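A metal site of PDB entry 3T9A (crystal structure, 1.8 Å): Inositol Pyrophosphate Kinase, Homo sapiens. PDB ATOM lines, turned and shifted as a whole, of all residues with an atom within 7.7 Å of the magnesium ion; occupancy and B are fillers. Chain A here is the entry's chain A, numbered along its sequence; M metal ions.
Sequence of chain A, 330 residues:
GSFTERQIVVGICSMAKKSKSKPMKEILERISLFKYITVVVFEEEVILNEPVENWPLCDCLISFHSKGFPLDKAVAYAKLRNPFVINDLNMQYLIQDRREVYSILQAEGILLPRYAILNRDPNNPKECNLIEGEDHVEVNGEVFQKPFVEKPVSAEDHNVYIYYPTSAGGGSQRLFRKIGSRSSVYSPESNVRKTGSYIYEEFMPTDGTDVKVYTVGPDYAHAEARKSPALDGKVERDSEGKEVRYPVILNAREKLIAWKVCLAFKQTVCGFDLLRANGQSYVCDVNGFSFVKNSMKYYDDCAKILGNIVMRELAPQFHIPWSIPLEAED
OD1 of Asn 87 sits close to O of Val 269 (2.9 Å).
OG1 of Thr 268 is in hydrogen-bond range of O of Ile 86, at 2.7 Å.
The side-chain amide oxygen (OE1) of Gln 267 sits close to the backbone carbonyl oxygen (O) of Phe 265, 2.9 Å away.
ND2 of Asn 87 lies close to N of Thr 268.
SG of Cys 262 lies close to O of Thr 268, 3.8 Å away.
NE2 of Gln 267 lies within hydrogen-bond range of OD1 of Asn 87 (2.9 Å).
The backbone NH (N) of Thr 215 lies within hydrogen-bond range of the backbone carbonyl oxygen (O) of Cys 270 (2.8 Å).
The backbone carbonyl oxygen (O) of Thr 268 sits close to the backbone NH (N) of Gly 217.
Val 269 touches the magnesium ion.
Cys 270 touches the magnesium ion.
Six residues have an atom within 4 Å of the magnesium ion: Thr 215, Cys 262, Gln 267, Thr 268, Val 269 and Cys 270.
The nearest printed residue that does not touch the magnesium ion is Gly 217 (4.4 Å).
The magnesium ion is bound by the side-chain hydroxyl (OG1) of Thr 215 (1.8 Å), the backbone carbonyl oxygen (O) of Gln 267 (2.3 Å) and the backbone carbonyl oxygen (O) of Thr 268 (2.5 Å).
The magnesium ion has three donor atoms within binding distance.
Slightly farther from the magnesium ion lies SG of Cys 262 (2.8 Å).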
ATOM      1  N   ILE A  86      -8.561 -34.724  15.456  1.00  0.00           N
ATOM      2  CA  ILE A  86      -7.886 -33.882  16.468  1.00  0.00           C
ATOM      3  C   ILE A  86      -6.735 -33.047  15.859  1.00  0.00           C
ATOM      4  O   ILE A  86      -6.624 -31.829  16.093  1.00  0.00           O
ATOM      5  CB  ILE A  86      -7.430 -34.768  17.674  1.00  0.00           C
ATOM      6  CG1 ILE A  86      -8.650 -35.326  18.436  1.00  0.00           C
ATOM      7  CG2 ILE A  86      -6.480 -34.045  18.634  1.00  0.00           C
ATOM      8  CD1 ILE A  86      -9.560 -34.265  19.091  1.00  0.00           C
ATOM      9  N   ASN A  87      -5.874 -33.714  15.099  1.00  0.00           N
ATOM     10  CA  ASN A  87      -4.790 -33.072  14.349  1.00  0.00           C
ATOM     11  C   ASN A  87      -5.040 -33.239  12.853  1.00  0.00           C
ATOM     12  O   ASN A  87      -5.020 -34.368  12.344  1.00  0.00           O
ATOM     13  CB  ASN A  87      -3.448 -33.707  14.708  1.00  0.00           C
ATOM     14  CG  ASN A  87      -2.780 -33.077  15.939  1.00  0.00           C
ATOM     15  OD1 ASN A  87      -1.586 -32.737  15.905  1.00  0.00           O
ATOM     16  ND2 ASN A  87      -3.527 -32.969  17.030  1.00  0.00           N
ATOM     17  N   TYR A 214       4.667 -26.828  23.940  1.00  0.00           N
ATOM     18  CA  TYR A 214       3.798 -27.988  23.684  1.00  0.00           C
ATOM     19  C   TYR A 214       2.355 -27.575  23.969  1.00  0.00           C
ATOM     20  O   TYR A 214       1.989 -27.300  25.139  1.00  0.00           O
ATOM     21  CB  TYR A 214       4.178 -29.156  24.604  1.00  0.00           C
ATOM     22  CG  TYR A 214       5.618 -29.604  24.459  1.00  0.00           C
ATOM     23  CD1 TYR A 214       6.667 -28.885  25.057  1.00  0.00           C
ATOM     24  CD2 TYR A 214       5.937 -30.755  23.725  1.00  0.00           C
ATOM     25  CE1 TYR A 214       7.988 -29.299  24.916  1.00  0.00           C
ATOM     26  CE2 TYR A 214       7.276 -31.179  23.583  1.00  0.00           C
ATOM     27  CZ  TYR A 214       8.278 -30.442  24.175  1.00  0.00           C
ATOM     28  OH  TYR A 214       9.597 -30.839  24.048  1.00  0.00           O
ATOM     29  N   THR A 215       1.540 -27.512  22.908  1.00  0.00           N
ATOM     30  CA  THR A 215       0.142 -27.112  23.044  1.00  0.00           C
ATOM     31  C   THR A 215      -0.753 -28.341  23.132  1.00  0.00           C
ATOM     32  O   THR A 215      -0.416 -29.411  22.613  1.00  0.00           O
ATOM     33  CB  THR A 215      -0.358 -26.227  21.888  1.00  0.00           C
ATOM     34  OG1 THR A 215      -0.622 -27.018  20.717  1.00  0.00           O
ATOM     35  CG2 THR A 215       0.628 -25.106  21.540  1.00  0.00           C
ATOM     36  N   VAL A 216      -1.885 -28.177  23.814  1.00  0.00           N
ATOM     37  CA  VAL A 216      -2.969 -29.159  23.765  1.00  0.00           C
ATOM     38  C   VAL A 216      -4.203 -28.300  23.611  1.00  0.00           C
ATOM     39  O   VAL A 216      -4.820 -27.848  24.607  1.00  0.00           O
ATOM     40  CB  VAL A 216      -3.072 -30.005  25.045  1.00  0.00           C
ATOM     41  CG1 VAL A 216      -4.136 -31.108  24.864  1.00  0.00           C
ATOM     42  CG2 VAL A 216      -1.697 -30.585  25.441  1.00  0.00           C
ATOM     43  N   GLY A 217      -4.527 -28.019  22.353  1.00  0.00           N
ATOM     44  CA  GLY A 217      -5.489 -26.989  22.024  1.00  0.00           C
ATOM     45  C   GLY A 217      -4.867 -25.609  22.193  1.00  0.00           C
ATOM     46  O   GLY A 217      -3.773 -25.447  22.755  1.00  0.00           O
ATOM     47  N   PRO A 218      -5.564 -24.584  21.682  1.00  0.00           N
ATOM     48  CA  PRO A 218      -4.985 -23.244  21.575  1.00  0.00           C
ATOM     49  C   PRO A 218      -4.882 -22.506  22.924  1.00  0.00           C
ATOM     50  O   PRO A 218      -4.086 -21.552  23.039  1.00  0.00           O
ATOM     51  CB  PRO A 218      -5.925 -22.524  20.604  1.00  0.00           C
ATOM     52  CG  PRO A 218      -7.190 -23.223  20.689  1.00  0.00           C
ATOM     53  CD  PRO A 218      -6.875 -24.677  21.006  1.00  0.00           C
ATOM     54  N   ASP A 219      -5.631 -22.952  23.931  1.00  0.00           N
ATOM     55  CA  ASP A 219      -5.613 -22.304  25.257  1.00  0.00           C
ATOM     56  C   ASP A 219      -4.786 -23.029  26.328  1.00  0.00           C
ATOM     57  O   ASP A 219      -4.900 -22.692  27.517  1.00  0.00           O
ATOM     58  CB  ASP A 219      -7.054 -22.109  25.746  1.00  0.00           C
ATOM     59  CG  ASP A 219      -7.836 -21.171  24.852  1.00  0.00           C
ATOM     60  OD1 ASP A 219      -7.236 -20.219  24.319  1.00  0.00           O
ATOM     61  OD2 ASP A 219      -9.070 -21.363  24.687  1.00  0.00           O
ATOM     62  N   TYR A 220      -3.966 -23.999  25.933  1.00  0.00           N
ATOM     63  CA  TYR A 220      -3.062 -24.658  26.871  1.00  0.00           C
ATOM     64  C   TYR A 220      -1.691 -24.826  26.228  1.00  0.00           C
ATOM     65  O   TYR A 220      -1.566 -25.440  25.177  1.00  0.00           O
ATOM     66  CB  TYR A 220      -3.601 -26.029  27.303  1.00  0.00           C
ATOM     67  CG  TYR A 220      -2.711 -26.778  28.266  1.00  0.00           C
ATOM     68  CD1 TYR A 220      -1.660 -27.575  27.796  1.00  0.00           C
ATOM     69  CD2 TYR A 220      -2.898 -26.689  29.652  1.00  0.00           C
ATOM     70  CE1 TYR A 220      -0.834 -28.269  28.677  1.00  0.00           C
ATOM     71  CE2 TYR A 220      -2.082 -27.378  30.534  1.00  0.00           C
ATOM     72  CZ  TYR A 220      -1.048 -28.165  30.050  1.00  0.00           C
ATOM     73  OH  TYR A 220      -0.237 -28.843  30.925  1.00  0.00           O
ATOM     74  N   ALA A 258       1.466 -19.295  20.788  1.00  0.00           N
ATOM     75  CA  ALA A 258       1.017 -20.692  20.920  1.00  0.00           C
ATOM     76  C   ALA A 258      -0.418 -20.891  20.375  1.00  0.00           C
ATOM     77  O   ALA A 258      -0.693 -21.859  19.671  1.00  0.00           O
ATOM     78  CB  ALA A 258       1.138 -21.165  22.365  1.00  0.00           C
ATOM     79  N   TRP A 259      -1.311 -19.968  20.734  1.00  0.00           N
ATOM     80  CA  TRP A 259      -2.696 -19.979  20.260  1.00  0.00           C
ATOM     81  C   TRP A 259      -2.740 -19.958  18.719  1.00  0.00           C
ATOM     82  O   TRP A 259      -3.447 -20.761  18.091  1.00  0.00           O
ATOM     83  CB  TRP A 259      -3.409 -18.766  20.847  1.00  0.00           C
ATOM     84  CG  TRP A 259      -4.874 -18.622  20.506  1.00  0.00           C
ATOM     85  CD1 TRP A 259      -5.932 -19.090  21.213  1.00  0.00           C
ATOM     86  CD2 TRP A 259      -5.414 -17.934  19.380  1.00  0.00           C
ATOM     87  NE1 TRP A 259      -7.121 -18.760  20.585  1.00  0.00           N
ATOM     88  CE2 TRP A 259      -6.828 -18.033  19.461  1.00  0.00           C
ATOM     89  CE3 TRP A 259      -4.853 -17.243  18.293  1.00  0.00           C
ATOM     90  CZ2 TRP A 259      -7.681 -17.467  18.505  1.00  0.00           C
ATOM     91  CZ3 TRP A 259      -5.701 -16.688  17.343  1.00  0.00           C
ATOM     92  CH2 TRP A 259      -7.108 -16.800  17.459  1.00  0.00           C
ATOM     93  N   VAL A 261      -0.178 -20.662  16.481  1.00  0.00           N
ATOM     94  CA  VAL A 261       0.457 -21.806  15.848  1.00  0.00           C
ATOM     95  C   VAL A 261      -0.476 -23.035  15.845  1.00  0.00           C
ATOM     96  O   VAL A 261      -0.646 -23.688  14.818  1.00  0.00           O
ATOM     97  CB  VAL A 261       1.811 -22.132  16.516  1.00  0.00           C
ATOM     98  CG1 VAL A 261       2.292 -23.528  16.124  1.00  0.00           C
ATOM     99  CG2 VAL A 261       2.826 -21.058  16.108  1.00  0.00           C
ATOM    100  N   CYS A 262      -1.099 -23.304  16.991  1.00  0.00           N
ATOM    101  CA  CYS A 262      -2.052 -24.413  17.120  1.00  0.00           C
ATOM    102  C   CYS A 262      -3.183 -24.321  16.079  1.00  0.00           C
ATOM    103  O   CYS A 262      -3.507 -25.294  15.376  1.00  0.00           O
ATOM    104  CB  CYS A 262      -2.612 -24.442  18.550  1.00  0.00           C
ATOM    105  SG  CYS A 262      -3.843 -25.693  18.862  1.00  0.00           S
ATOM    106  N   LEU A 263      -3.790 -23.140  15.991  1.00  0.00           N
ATOM    107  CA  LEU A 263      -4.887 -22.933  15.046  1.00  0.00           C
ATOM    108  C   LEU A 263      -4.453 -22.881  13.576  1.00  0.00           C
ATOM    109  O   LEU A 263      -5.126 -23.461  12.723  1.00  0.00           O
ATOM    110  CB  LEU A 263      -5.742 -21.717  15.451  1.00  0.00           C
ATOM    111  CG  LEU A 263      -6.460 -21.923  16.799  1.00  0.00           C
ATOM    112  CD1 LEU A 263      -6.966 -20.624  17.393  1.00  0.00           C
ATOM    113  CD2 LEU A 263      -7.641 -22.930  16.652  1.00  0.00           C
ATOM    114  N   PHE A 265      -1.916 -24.230  12.044  1.00  0.00           N
ATOM    115  CA  PHE A 265      -1.540 -25.541  11.550  1.00  0.00           C
ATOM    116  C   PHE A 265      -2.606 -26.615  11.803  1.00  0.00           C
ATOM    117  O   PHE A 265      -2.423 -27.766  11.425  1.00  0.00           O
ATOM    118  CB  PHE A 265      -0.178 -25.951  12.144  1.00  0.00           C
ATOM    119  CG  PHE A 265       0.967 -25.131  11.619  1.00  0.00           C
ATOM    120  CD1 PHE A 265       1.626 -25.496  10.449  1.00  0.00           C
ATOM    121  CD2 PHE A 265       1.355 -23.957  12.265  1.00  0.00           C
ATOM    122  CE1 PHE A 265       2.681 -24.716   9.945  1.00  0.00           C
ATOM    123  CE2 PHE A 265       2.401 -23.173  11.762  1.00  0.00           C
ATOM    124  CZ  PHE A 265       3.071 -23.560  10.605  1.00  0.00           C
ATOM    125  N   LYS A 266      -3.705 -26.225  12.450  1.00  0.00           N
ATOM    126  CA  LYS A 266      -4.795 -27.159  12.778  1.00  0.00           C
ATOM    127  C   LYS A 266      -4.305 -28.407  13.517  1.00  0.00           C
ATOM    128  O   LYS A 266      -4.822 -29.513  13.307  1.00  0.00           O
ATOM    129  CB  LYS A 266      -5.545 -27.563  11.501  1.00  0.00           C
ATOM    130  CG  LYS A 266      -6.193 -26.413  10.740  1.00  0.00           C
ATOM    131  CD  LYS A 266      -6.828 -26.937   9.435  1.00  0.00           C
ATOM    132  CE  LYS A 266      -7.075 -25.792   8.455  1.00  0.00           C
ATOM    133  NZ  LYS A 266      -7.186 -26.273   7.038  1.00  0.00           N
ATOM    134  N   GLN A 267      -3.294 -28.248  14.371  1.00  0.00           N
ATOM    135  CA  GLN A 267      -2.783 -29.379  15.142  1.00  0.00           C
ATOM    136  C   GLN A 267      -3.103 -29.163  16.613  1.00  0.00           C
ATOM    137  O   GLN A 267      -2.353 -28.475  17.299  1.00  0.00           O
ATOM    138  CB  GLN A 267      -1.259 -29.549  14.964  1.00  0.00           C
ATOM    139  CG  GLN A 267      -0.762 -29.630  13.516  1.00  0.00           C
ATOM    140  CD  GLN A 267      -1.338 -30.826  12.745  1.00  0.00           C
ATOM    141  OE1 GLN A 267      -2.119 -30.648  11.808  1.00  0.00           O
ATOM    142  NE2 GLN A 267      -0.956 -32.020  13.148  1.00  0.00           N
ATOM    143  N   THR A 268      -4.201 -29.732  17.104  1.00  0.00           N
ATOM    144  CA  THR A 268      -4.532 -29.638  18.542  1.00  0.00           C
ATOM    145  C   THR A 268      -3.299 -29.887  19.441  1.00  0.00           C
ATOM    146  O   THR A 268      -2.952 -29.069  20.287  1.00  0.00           O
ATOM    147  CB  THR A 268      -5.695 -30.605  18.920  1.00  0.00           C
ATOM    148  OG1 THR A 268      -6.871 -30.222  18.188  1.00  0.00           O
ATOM    149  CG2 THR A 268      -5.984 -30.585  20.440  1.00  0.00           C
ATOM    150  N   VAL A 269      -2.635 -31.028  19.247  1.00  0.00           N
ATOM    151  CA  VAL A 269      -1.411 -31.324  19.981  1.00  0.00           C
ATOM    152  C   VAL A 269      -0.260 -30.901  19.059  1.00  0.00           C
ATOM    153  O   VAL A 269      -0.071 -31.502  18.008  1.00  0.00           O
ATOM    154  CB  VAL A 269      -1.303 -32.842  20.312  1.00  0.00           C
ATOM    155  CG1 VAL A 269       0.000 -33.143  21.095  1.00  0.00           C
ATOM    156  CG2 VAL A 269      -2.546 -33.339  21.077  1.00  0.00           C
ATOM    157  N   CYS A 270       0.481 -29.835  19.427  1.00  0.00           N
ATOM    158  CA  CYS A 270       1.549 -29.319  18.567  1.00  0.00           C
ATOM    159  C   CYS A 270       2.764 -28.852  19.386  1.00  0.00           C
ATOM    160  O   CYS A 270       2.596 -28.190  20.418  1.00  0.00           O
ATOM    161  CB  CYS A 270       1.013 -28.147  17.720  1.00  0.00           C
ATOM    162  SG  CYS A 270       2.023 -27.617  16.337  1.00  0.00           S
ATOM    163  N   GLY A 271       3.952 -29.175  18.917  1.00  0.00           N
ATOM    164  CA  GLY A 271       5.158 -28.649  19.541  1.00  0.00           C
ATOM    165  C   GLY A 271       5.787 -27.660  18.578  1.00  0.00           C
ATOM    166  O   GLY A 271       5.754 -27.866  17.353  1.00  0.00           O
ATOM    167  N   PHE A 272       6.362 -26.595  19.111  1.00  0.00           N
ATOM    168  CA  PHE A 272       7.181 -25.683  18.297  1.00  0.00           C
ATOM    169  C   PHE A 272       8.293 -25.096  19.165  1.00  0.00           C
ATOM    170  O   PHE A 272       8.241 -25.207  20.386  1.00  0.00           O
ATOM    171  CB  PHE A 272       6.331 -24.593  17.629  1.00  0.00           C
ATOM    172  CG  PHE A 272       5.655 -23.646  18.580  1.00  0.00           C
ATOM    173  CD1 PHE A 272       4.407 -23.972  19.111  1.00  0.00           C
ATOM    174  CD2 PHE A 272       6.265 -22.425  18.928  1.00  0.00           C
ATOM    175  CE1 PHE A 272       3.760 -23.112  20.009  1.00  0.00           C
ATOM    176  CE2 PHE A 272       5.633 -21.558  19.826  1.00  0.00           C
ATOM    177  CZ  PHE A 272       4.358 -21.892  20.350  1.00  0.00           C
ATOM    178  N   GLY A 288       4.632 -30.180  14.822  1.00  0.00           N
ATOM    179  CA  GLY A 288       3.392 -30.932  14.855  1.00  0.00           C
ATOM    180  C   GLY A 288       3.267 -31.757  16.128  1.00  0.00           C
ATOM    181  O   GLY A 288       3.835 -31.398  17.159  1.00  0.00           O
ATOM    182  N   PHE A 289       2.557 -32.865  16.027  1.00  0.00           N
ATOM    183  CA  PHE A 289       2.258 -33.726  17.168  1.00  0.00           C
ATOM    184  C   PHE A 289       3.477 -34.040  18.029  1.00  0.00           C
ATOM    185  O   PHE A 289       4.462 -34.646  17.560  1.00  0.00           O
ATOM    186  CB  PHE A 289       1.573 -35.016  16.734  1.00  0.00           C
ATOM    187  CG  PHE A 289       0.791 -35.673  17.818  1.00  0.00           C
ATOM    188  CD1 PHE A 289       1.444 -36.436  18.799  1.00  0.00           C
ATOM    189  CD2 PHE A 289      -0.594 -35.553  17.872  1.00  0.00           C
ATOM    190  CE1 PHE A 289       0.726 -37.053  19.806  1.00  0.00           C
ATOM    191  CE2 PHE A 289      -1.312 -36.170  18.879  1.00  0.00           C
ATOM    192  CZ  PHE A 289      -0.652 -36.920  19.846  1.00  0.00           C
HETATM  193 MG    MG M   1      -1.575 -27.359  19.183  1.00  0.00          MG
